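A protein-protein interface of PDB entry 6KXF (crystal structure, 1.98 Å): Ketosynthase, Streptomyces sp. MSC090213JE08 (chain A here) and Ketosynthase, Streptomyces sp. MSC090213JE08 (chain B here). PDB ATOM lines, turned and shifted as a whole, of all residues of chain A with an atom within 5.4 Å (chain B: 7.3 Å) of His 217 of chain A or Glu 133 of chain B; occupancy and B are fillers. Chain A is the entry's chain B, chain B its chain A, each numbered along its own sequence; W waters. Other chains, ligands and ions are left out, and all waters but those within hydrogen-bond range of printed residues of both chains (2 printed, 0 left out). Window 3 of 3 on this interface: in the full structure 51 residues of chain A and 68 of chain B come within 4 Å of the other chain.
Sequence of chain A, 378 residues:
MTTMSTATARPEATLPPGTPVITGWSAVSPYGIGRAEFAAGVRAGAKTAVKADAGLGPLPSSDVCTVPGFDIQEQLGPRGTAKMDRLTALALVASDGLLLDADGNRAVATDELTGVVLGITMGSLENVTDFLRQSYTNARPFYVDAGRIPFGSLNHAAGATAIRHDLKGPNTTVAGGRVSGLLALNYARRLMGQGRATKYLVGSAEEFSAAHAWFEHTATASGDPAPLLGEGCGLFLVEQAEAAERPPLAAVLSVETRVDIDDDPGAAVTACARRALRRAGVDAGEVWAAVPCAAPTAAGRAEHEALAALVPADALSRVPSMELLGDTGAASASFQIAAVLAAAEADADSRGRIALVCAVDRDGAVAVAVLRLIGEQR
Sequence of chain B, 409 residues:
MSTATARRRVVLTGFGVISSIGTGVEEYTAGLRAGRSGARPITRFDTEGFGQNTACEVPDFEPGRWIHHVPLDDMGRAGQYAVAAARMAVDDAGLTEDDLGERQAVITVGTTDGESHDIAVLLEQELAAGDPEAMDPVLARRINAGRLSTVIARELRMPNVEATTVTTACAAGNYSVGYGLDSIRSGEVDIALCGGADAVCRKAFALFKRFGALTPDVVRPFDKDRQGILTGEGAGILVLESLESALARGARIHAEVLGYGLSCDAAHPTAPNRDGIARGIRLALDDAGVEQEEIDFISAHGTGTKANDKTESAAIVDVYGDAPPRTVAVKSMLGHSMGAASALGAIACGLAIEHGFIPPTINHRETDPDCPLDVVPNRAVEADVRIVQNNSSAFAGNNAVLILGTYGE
A ring nitrogen (NE2) of His 217 of chain A is in hydrogen-bond range of the side-chain carboxylate of Glu 133 of chain B (2.8 Å).
The side-chain amide oxygen (OE1) of Gln 125 of chain B lies within hydrogen-bond range of the backbone NH (N) of Asp 136 of chain B (3.0 Å). The side-chain carboxylate of Asp 131 of chain B lies close to the backbone NH of Glu 133 of chain B (3.3 Å). OG1 of Thr 218 of chain A is in hydrogen-bond range of O of Trp 214 of chain A, at 2.7 Å.
CE3 of Trp 214 of chain A touches CB of Pro 132 of chain B (3.6 Å). Trp 214 of chain A touches Glu 133 of chain B (CZ3 to OE2, 3.9 Å). Met 135 of chain B touches Phe 215 of chain A (SD to CE1, 3.8 Å). Ala 140 of chain B touches Phe 215 of chain A. Met 135 of chain B touches Thr 218 of chain A. CG2 of Thr 218 of chain A touches O of Asp 136 of chain B, at 3.7 Å. Thr 218 of chain A touches Pro 137 of chain B (O to CB, 3.4 Å). Thr 218 of chain A touches Ala 140 of chain B.
Of chain B, only Glu 133 (2.8 Å) comes within 4 Å of His 217 of chain A. Glu 133 of chain B touches just these residues of chain A: Trp 214 and His 217. Printed residues of chain A within 4 Å of Pro 132 of chain B: Trp 214 (3.6 Å). Of the printed residues of chain A, Ala 140 of chain B touches Phe 215 (3.8 Å) and Thr 218 (3.7 Å). Printed residues of chain A within 4 Å of Met 135 of chain B: Phe 215 and Thr 218. Glu 216 of chain A touches none of the printed residues of chain B. The nearest residue of chain B that does not touch His 217 of chain A is Pro 132 of chain B (5.9 Å). The nearest printed residue of chain A that does not touch Glu 133 of chain B is Pro 60 of chain A (6.0 Å).
Of the 11 printed residues of chain A, 4 touch a printed residue of chain B. Of the 12 printed residues of chain B, 6 touch a printed residue of chain A. Hydrophobic or aromatic side chains of chain B within 4 Å of the printed part of chain A: Pro 132, Met 135, Pro 137 and Ala 140. Among the printed residues, no Asp or Glu carboxylate lies within 4 Å of a Lys or Arg side-chain nitrogen of the other chain.
Water W1 lies within hydrogen-bond range of the side-chain hydroxyl (OG1) of Thr 218 of chain A (2.7 Å) and the backbone carbonyl oxygen (O) of Pro 132 of chain B (2.9 Å). Water W2 lies within hydrogen-bond range of the side-chain carboxylate of Glu 216 of chain A (2.9 Å) and the backbone carbonyl oxygen of Ala 140 of chain B (3.4 Å).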
ATOM      1  N   PRO A  60      17.017  10.086 -30.623  1.00  0.00           N
ATOM      2  CA  PRO A  60      18.377  10.196 -31.155  1.00  0.00           C
ATOM      3  C   PRO A  60      18.468  10.502 -32.652  1.00  0.00           C
ATOM      4  O   PRO A  60      19.439  11.096 -33.101  1.00  0.00           O
ATOM      5  CB  PRO A  60      18.970   8.797 -30.966  1.00  0.00           C
ATOM      6  CG  PRO A  60      17.752   7.883 -30.951  1.00  0.00           C
ATOM      7  CD  PRO A  60      16.656   8.697 -30.292  1.00  0.00           C
ATOM      8  N   HIS A 212      13.590   2.280 -26.605  1.00  0.00           N
ATOM      9  CA  HIS A 212      14.229   1.402 -27.557  1.00  0.00           C
ATOM     10  C   HIS A 212      15.183   2.203 -28.463  1.00  0.00           C
ATOM     11  O   HIS A 212      16.299   1.747 -28.726  1.00  0.00           O
ATOM     12  CB  HIS A 212      13.190   0.606 -28.367  1.00  0.00           C
ATOM     13  CG  HIS A 212      13.783  -0.331 -29.372  1.00  0.00           C
ATOM     14  ND1 HIS A 212      14.958  -1.010 -29.165  1.00  0.00           N
ATOM     15  CD2 HIS A 212      13.381  -0.677 -30.617  1.00  0.00           C
ATOM     16  CE1 HIS A 212      15.249  -1.757 -30.222  1.00  0.00           C
ATOM     17  NE2 HIS A 212      14.290  -1.585 -31.129  1.00  0.00           N
ATOM     18  N   ALA A 213      14.749   3.382 -28.923  1.00  0.00           N
ATOM     19  CA  ALA A 213      15.563   4.186 -29.854  1.00  0.00           C
ATOM     20  C   ALA A 213      16.859   4.592 -29.145  1.00  0.00           C
ATOM     21  O   ALA A 213      17.949   4.337 -29.628  1.00  0.00           O
ATOM     22  CB  ALA A 213      14.788   5.391 -30.347  1.00  0.00           C
ATOM     23  N   TRP A 214      16.718   5.143 -27.950  1.00  0.00           N
ATOM     24  CA  TRP A 214      17.848   5.598 -27.150  1.00  0.00           C
ATOM     25  C   TRP A 214      18.791   4.464 -26.720  1.00  0.00           C
ATOM     26  O   TRP A 214      20.027   4.677 -26.645  1.00  0.00           O
ATOM     27  CB  TRP A 214      17.325   6.367 -25.949  1.00  0.00           C
ATOM     28  CG  TRP A 214      16.980   7.778 -26.291  1.00  0.00           C
ATOM     29  CD1 TRP A 214      15.751   8.368 -26.284  1.00  0.00           C
ATOM     30  CD2 TRP A 214      17.917   8.777 -26.716  1.00  0.00           C
ATOM     31  NE1 TRP A 214      15.870   9.680 -26.647  1.00  0.00           N
ATOM     32  CE2 TRP A 214      17.182   9.958 -26.928  1.00  0.00           C
ATOM     33  CE3 TRP A 214      19.303   8.782 -26.929  1.00  0.00           C
ATOM     34  CZ2 TRP A 214      17.796  11.147 -27.323  1.00  0.00           C
ATOM     35  CZ3 TRP A 214      19.909   9.953 -27.332  1.00  0.00           C
ATOM     36  CH2 TRP A 214      19.161  11.121 -27.514  1.00  0.00           C
ATOM     37  N   PHE A 215      18.263   3.264 -26.452  1.00  0.00           N
ATOM     38  CA  PHE A 215      19.164   2.112 -26.101  1.00  0.00           C
ATOM     39  C   PHE A 215      19.951   1.686 -27.343  1.00  0.00           C
ATOM     40  O   PHE A 215      21.151   1.343 -27.208  1.00  0.00           O
ATOM     41  CB  PHE A 215      18.430   0.889 -25.513  1.00  0.00           C
ATOM     42  CG  PHE A 215      17.877   1.058 -24.118  1.00  0.00           C
ATOM     43  CD1 PHE A 215      18.503   1.871 -23.185  1.00  0.00           C
ATOM     44  CD2 PHE A 215      16.701   0.432 -23.746  1.00  0.00           C
ATOM     45  CE1 PHE A 215      17.985   2.032 -21.906  1.00  0.00           C
ATOM     46  CE2 PHE A 215      16.174   0.615 -22.479  1.00  0.00           C
ATOM     47  CZ  PHE A 215      16.825   1.404 -21.557  1.00  0.00           C
ATOM     48  N   GLU A 216      19.290   1.664 -28.515  1.00  0.00           N
ATOM     49  CA  GLU A 216      19.950   1.247 -29.778  1.00  0.00           C
ATOM     50  C   GLU A 216      21.075   2.244 -30.137  1.00  0.00           C
ATOM     51  O   GLU A 216      22.158   1.833 -30.610  1.00  0.00           O
ATOM     52  CB  GLU A 216      18.960   1.129 -30.943  1.00  0.00           C
ATOM     53  CG  GLU A 216      18.119  -0.130 -30.908  1.00  0.00           C
ATOM     54  CD  GLU A 216      18.938  -1.405 -30.969  1.00  0.00           C
ATOM     55  OE1 GLU A 216      19.552  -1.639 -32.012  1.00  0.00           O
ATOM     56  OE2 GLU A 216      18.992  -2.127 -29.953  1.00  0.00           O
ATOM     57  N   HIS A 217      20.809   3.526 -29.877  1.00  0.00           N
ATOM     58  CA  HIS A 217      21.747   4.644 -30.091  1.00  0.00           C
ATOM     59  C   HIS A 217      22.969   4.475 -29.181  1.00  0.00           C
ATOM     60  O   HIS A 217      24.108   4.501 -29.672  1.00  0.00           O
ATOM     61  CB  HIS A 217      21.044   5.992 -29.854  1.00  0.00           C
ATOM     62  CG  HIS A 217      21.989   7.139 -29.835  1.00  0.00           C
ATOM     63  ND1 HIS A 217      22.683   7.529 -30.963  1.00  0.00           N
ATOM     64  CD2 HIS A 217      22.401   7.941 -28.826  1.00  0.00           C
ATOM     65  CE1 HIS A 217      23.459   8.547 -30.657  1.00  0.00           C
ATOM     66  NE2 HIS A 217      23.301   8.820 -29.353  1.00  0.00           N
ATOM     67  N   THR A 218      22.711   4.247 -27.878  1.00  0.00           N
ATOM     68  CA  THR A 218      23.728   4.003 -26.859  1.00  0.00           C
ATOM     69  C   THR A 218      24.645   2.842 -27.261  1.00  0.00           C
ATOM     70  O   THR A 218      25.838   2.888 -26.996  1.00  0.00           O
ATOM     71  CB  THR A 218      23.119   3.694 -25.485  1.00  0.00           C
ATOM     72  OG1 THR A 218      22.202   4.723 -25.118  1.00  0.00           O
ATOM     73  CG2 THR A 218      24.162   3.555 -24.404  1.00  0.00           C
ATOM     74  N   ALA A 219      24.077   1.821 -27.906  1.00  0.00           N
ATOM     75  CA  ALA A 219      24.789   0.590 -28.307  1.00  0.00           C
ATOM     76  C   ALA A 219      25.623   0.772 -29.591  1.00  0.00           C
ATOM     77  O   ALA A 219      26.420  -0.083 -29.918  1.00  0.00           O
ATOM     78  CB  ALA A 219      23.781  -0.522 -28.522  1.00  0.00           C
ATOM     79  N   THR A 220      25.361   1.833 -30.359  1.00  0.00           N
ATOM     80  CA  THR A 220      25.943   1.984 -31.692  1.00  0.00           C
ATOM     81  C   THR A 220      27.310   2.674 -31.554  1.00  0.00           C
ATOM     82  O   THR A 220      27.412   3.707 -30.932  1.00  0.00           O
ATOM     83  CB  THR A 220      24.981   2.748 -32.611  1.00  0.00           C
ATOM     84  OG1 THR A 220      23.726   2.078 -32.736  1.00  0.00           O
ATOM     85  CG2 THR A 220      25.542   2.901 -34.004  1.00  0.00           C
ATOM     86  N   PRO A 227      20.826   3.965 -36.217  1.00  0.00           N
ATOM     87  CA  PRO A 227      19.836   2.908 -36.449  1.00  0.00           C
ATOM     88  C   PRO A 227      18.593   3.494 -37.135  1.00  0.00           C
ATOM     89  O   PRO A 227      18.122   4.547 -36.733  1.00  0.00           O
ATOM     90  CB  PRO A 227      19.557   2.378 -35.032  1.00  0.00           C
ATOM     91  CG  PRO A 227      20.794   2.772 -34.234  1.00  0.00           C
ATOM     92  CD  PRO A 227      21.202   4.124 -34.808  1.00  0.00           C
ATOM     93  N   GLN B 125      22.003   6.564 -14.936  1.00  0.00           N
ATOM     94  CA  GLN B 125      23.062   7.326 -15.625  1.00  0.00           C
ATOM     95  C   GLN B 125      22.417   8.501 -16.382  1.00  0.00           C
ATOM     96  O   GLN B 125      22.886   9.636 -16.300  1.00  0.00           O
ATOM     97  CB  GLN B 125      23.863   6.395 -16.537  1.00  0.00           C
ATOM     98  CG  GLN B 125      24.700   5.375 -15.769  1.00  0.00           C
ATOM     99  CD  GLN B 125      25.197   4.234 -16.617  1.00  0.00           C
ATOM    100  OE1 GLN B 125      24.745   4.016 -17.740  1.00  0.00           O
ATOM    101  NE2 GLN B 125      26.137   3.475 -16.072  1.00  0.00           N
ATOM    102  N   GLU B 126      21.317   8.200 -17.079  1.00  0.00           N
ATOM    103  CA  GLU B 126      20.508   9.163 -17.756  1.00  0.00           C
ATOM    104  C   GLU B 126      20.050  10.238 -16.767  1.00  0.00           C
ATOM    105  O   GLU B 126      20.307  11.399 -17.027  1.00  0.00           O
ATOM    106  CB  GLU B 126      19.314   8.504 -18.449  1.00  0.00           C
ATOM    107  CG  GLU B 126      18.311   9.496 -19.011  1.00  0.00           C
ATOM    108  CD  GLU B 126      17.336   8.953 -20.047  1.00  0.00           C
ATOM    109  OE1 GLU B 126      17.422   7.752 -20.410  1.00  0.00           O
ATOM    110  OE2 GLU B 126      16.476   9.736 -20.490  1.00  0.00           O
ATOM    111  N   ALA B 129      22.738  12.646 -15.234  1.00  0.00           N
ATOM    112  CA  ALA B 129      23.290  13.627 -16.208  1.00  0.00           C
ATOM    113  C   ALA B 129      22.209  14.570 -16.777  1.00  0.00           C
ATOM    114  O   ALA B 129      22.541  15.609 -17.306  1.00  0.00           O
ATOM    115  CB  ALA B 129      23.983  12.891 -17.331  1.00  0.00           C
ATOM    116  N   GLY B 130      20.935  14.183 -16.685  1.00  0.00           N
ATOM    117  CA  GLY B 130      19.815  14.809 -17.375  1.00  0.00           C
ATOM    118  C   GLY B 130      19.873  14.566 -18.872  1.00  0.00           C
ATOM    119  O   GLY B 130      19.249  15.294 -19.648  1.00  0.00           O
ATOM    120  N   ASP B 131      20.601  13.519 -19.279  1.00  0.00           N
ATOM    121  CA  ASP B 131      20.994  13.326 -20.663  1.00  0.00           C
ATOM    122  C   ASP B 131      21.099  11.838 -21.004  1.00  0.00           C
ATOM    123  O   ASP B 131      21.945  11.133 -20.455  1.00  0.00           O
ATOM    124  CB  ASP B 131      22.333  14.019 -20.922  1.00  0.00           C
ATOM    125  CG  ASP B 131      22.649  14.195 -22.394  1.00  0.00           C
ATOM    126  OD1 ASP B 131      21.833  13.740 -23.227  1.00  0.00           O
ATOM    127  OD2 ASP B 131      23.707  14.801 -22.699  1.00  0.00           O
ATOM    128  N   PRO B 132      20.307  11.325 -21.975  1.00  0.00           N
ATOM    129  CA  PRO B 132      20.441   9.933 -22.401  1.00  0.00           C
ATOM    130  C   PRO B 132      21.841   9.565 -22.932  1.00  0.00           C
ATOM    131  O   PRO B 132      22.169   8.382 -22.954  1.00  0.00           O
ATOM    132  CB  PRO B 132      19.366   9.758 -23.484  1.00  0.00           C
ATOM    133  CG  PRO B 132      19.011  11.173 -23.911  1.00  0.00           C
ATOM    134  CD  PRO B 132      19.224  12.029 -22.683  1.00  0.00           C
ATOM    135  N   GLU B 133      22.659  10.561 -23.321  1.00  0.00           N
ATOM    136  CA  GLU B 133      24.004  10.326 -23.886  1.00  0.00           C
ATOM    137  C   GLU B 133      24.970   9.794 -22.822  1.00  0.00           C
ATOM    138  O   GLU B 133      25.951   9.198 -23.170  1.00  0.00           O
ATOM    139  CB  GLU B 133      24.597  11.611 -24.494  1.00  0.00           C
ATOM    140  CG  GLU B 133      23.949  12.055 -25.799  1.00  0.00           C
ATOM    141  CD  GLU B 133      24.152  11.125 -26.984  1.00  0.00           C
ATOM    142  OE1 GLU B 133      24.971  10.192 -26.881  1.00  0.00           O
ATOM    143  OE2 GLU B 133      23.469  11.319 -27.998  1.00  0.00           O
ATOM    144  N   ALA B 134      24.680  10.004 -21.531  1.00  0.00           N
ATOM    145  CA  ALA B 134      25.553   9.509 -20.430  1.00  0.00           C
ATOM    146  C   ALA B 134      25.390   7.984 -20.187  1.00  0.00           C
ATOM    147  O   ALA B 134      26.100   7.412 -19.367  1.00  0.00           O
ATOM    148  CB  ALA B 134      25.247  10.269 -19.170  1.00  0.00           C
ATOM    149  N   MET B 135      24.467   7.317 -20.884  1.00  0.00           N
ATOM    150  CA  MET B 135      24.268   5.871 -20.690  1.00  0.00           C
ATOM    151  C   MET B 135      25.465   5.090 -21.254  1.00  0.00           C
ATOM    152  O   MET B 135      26.015   5.382 -22.342  1.00  0.00           O
ATOM    153  CB  MET B 135      22.973   5.385 -21.347  1.00  0.00           C
ATOM    154  CG  MET B 135      21.725   5.859 -20.633  1.00  0.00           C
ATOM    155  SD  MET B 135      20.219   5.024 -21.214  1.00  0.00           S
ATOM    156  CE  MET B 135      19.899   5.831 -22.782  1.00  0.00           C
ATOM    157  N   ASP B 136      25.831   4.038 -20.521  1.00  0.00           N
ATOM    158  CA  ASP B 136      26.958   3.183 -20.851  1.00  0.00           C
ATOM    159  C   ASP B 136      26.617   2.201 -21.977  1.00  0.00           C
ATOM    160  O   ASP B 136      25.705   1.392 -21.870  1.00  0.00           O
ATOM    161  CB  ASP B 136      27.403   2.466 -19.591  1.00  0.00           C
ATOM    162  CG  ASP B 136      28.603   1.563 -19.751  1.00  0.00           C
ATOM    163  OD1 ASP B 136      29.189   1.495 -20.893  1.00  0.00           O
ATOM    164  OD2 ASP B 136      28.964   0.958 -18.716  1.00  0.00           O
ATOM    165  N   PRO B 137      27.364   2.221 -23.098  1.00  0.00           N
ATOM    166  CA  PRO B 137      27.180   1.232 -24.156  1.00  0.00           C
ATOM    167  C   PRO B 137      27.322  -0.249 -23.746  1.00  0.00           C
ATOM    168  O   PRO B 137      26.687  -1.115 -24.369  1.00  0.00           O
ATOM    169  CB  PRO B 137      28.312   1.586 -25.146  1.00  0.00           C
ATOM    170  CG  PRO B 137      28.592   3.055 -24.913  1.00  0.00           C
ATOM    171  CD  PRO B 137      28.396   3.233 -23.427  1.00  0.00           C
ATOM    172  N   ALA B 140      23.983  -1.204 -22.322  1.00  0.00           N
ATOM    173  CA  ALA B 140      22.913  -1.199 -23.315  1.00  0.00           C
ATOM    174  C   ALA B 140      23.027  -2.407 -24.240  1.00  0.00           C
ATOM    175  O   ALA B 140      22.016  -2.913 -24.662  1.00  0.00           O
ATOM    176  CB  ALA B 140      22.897   0.081 -24.108  1.00  0.00           C
HETATM  177  O   HOH W   1      23.521   7.120 -25.183  1.00  0.00           O
HETATM  178  O   HOH W   2      19.871  -2.518 -27.225  1.00  0.00           O
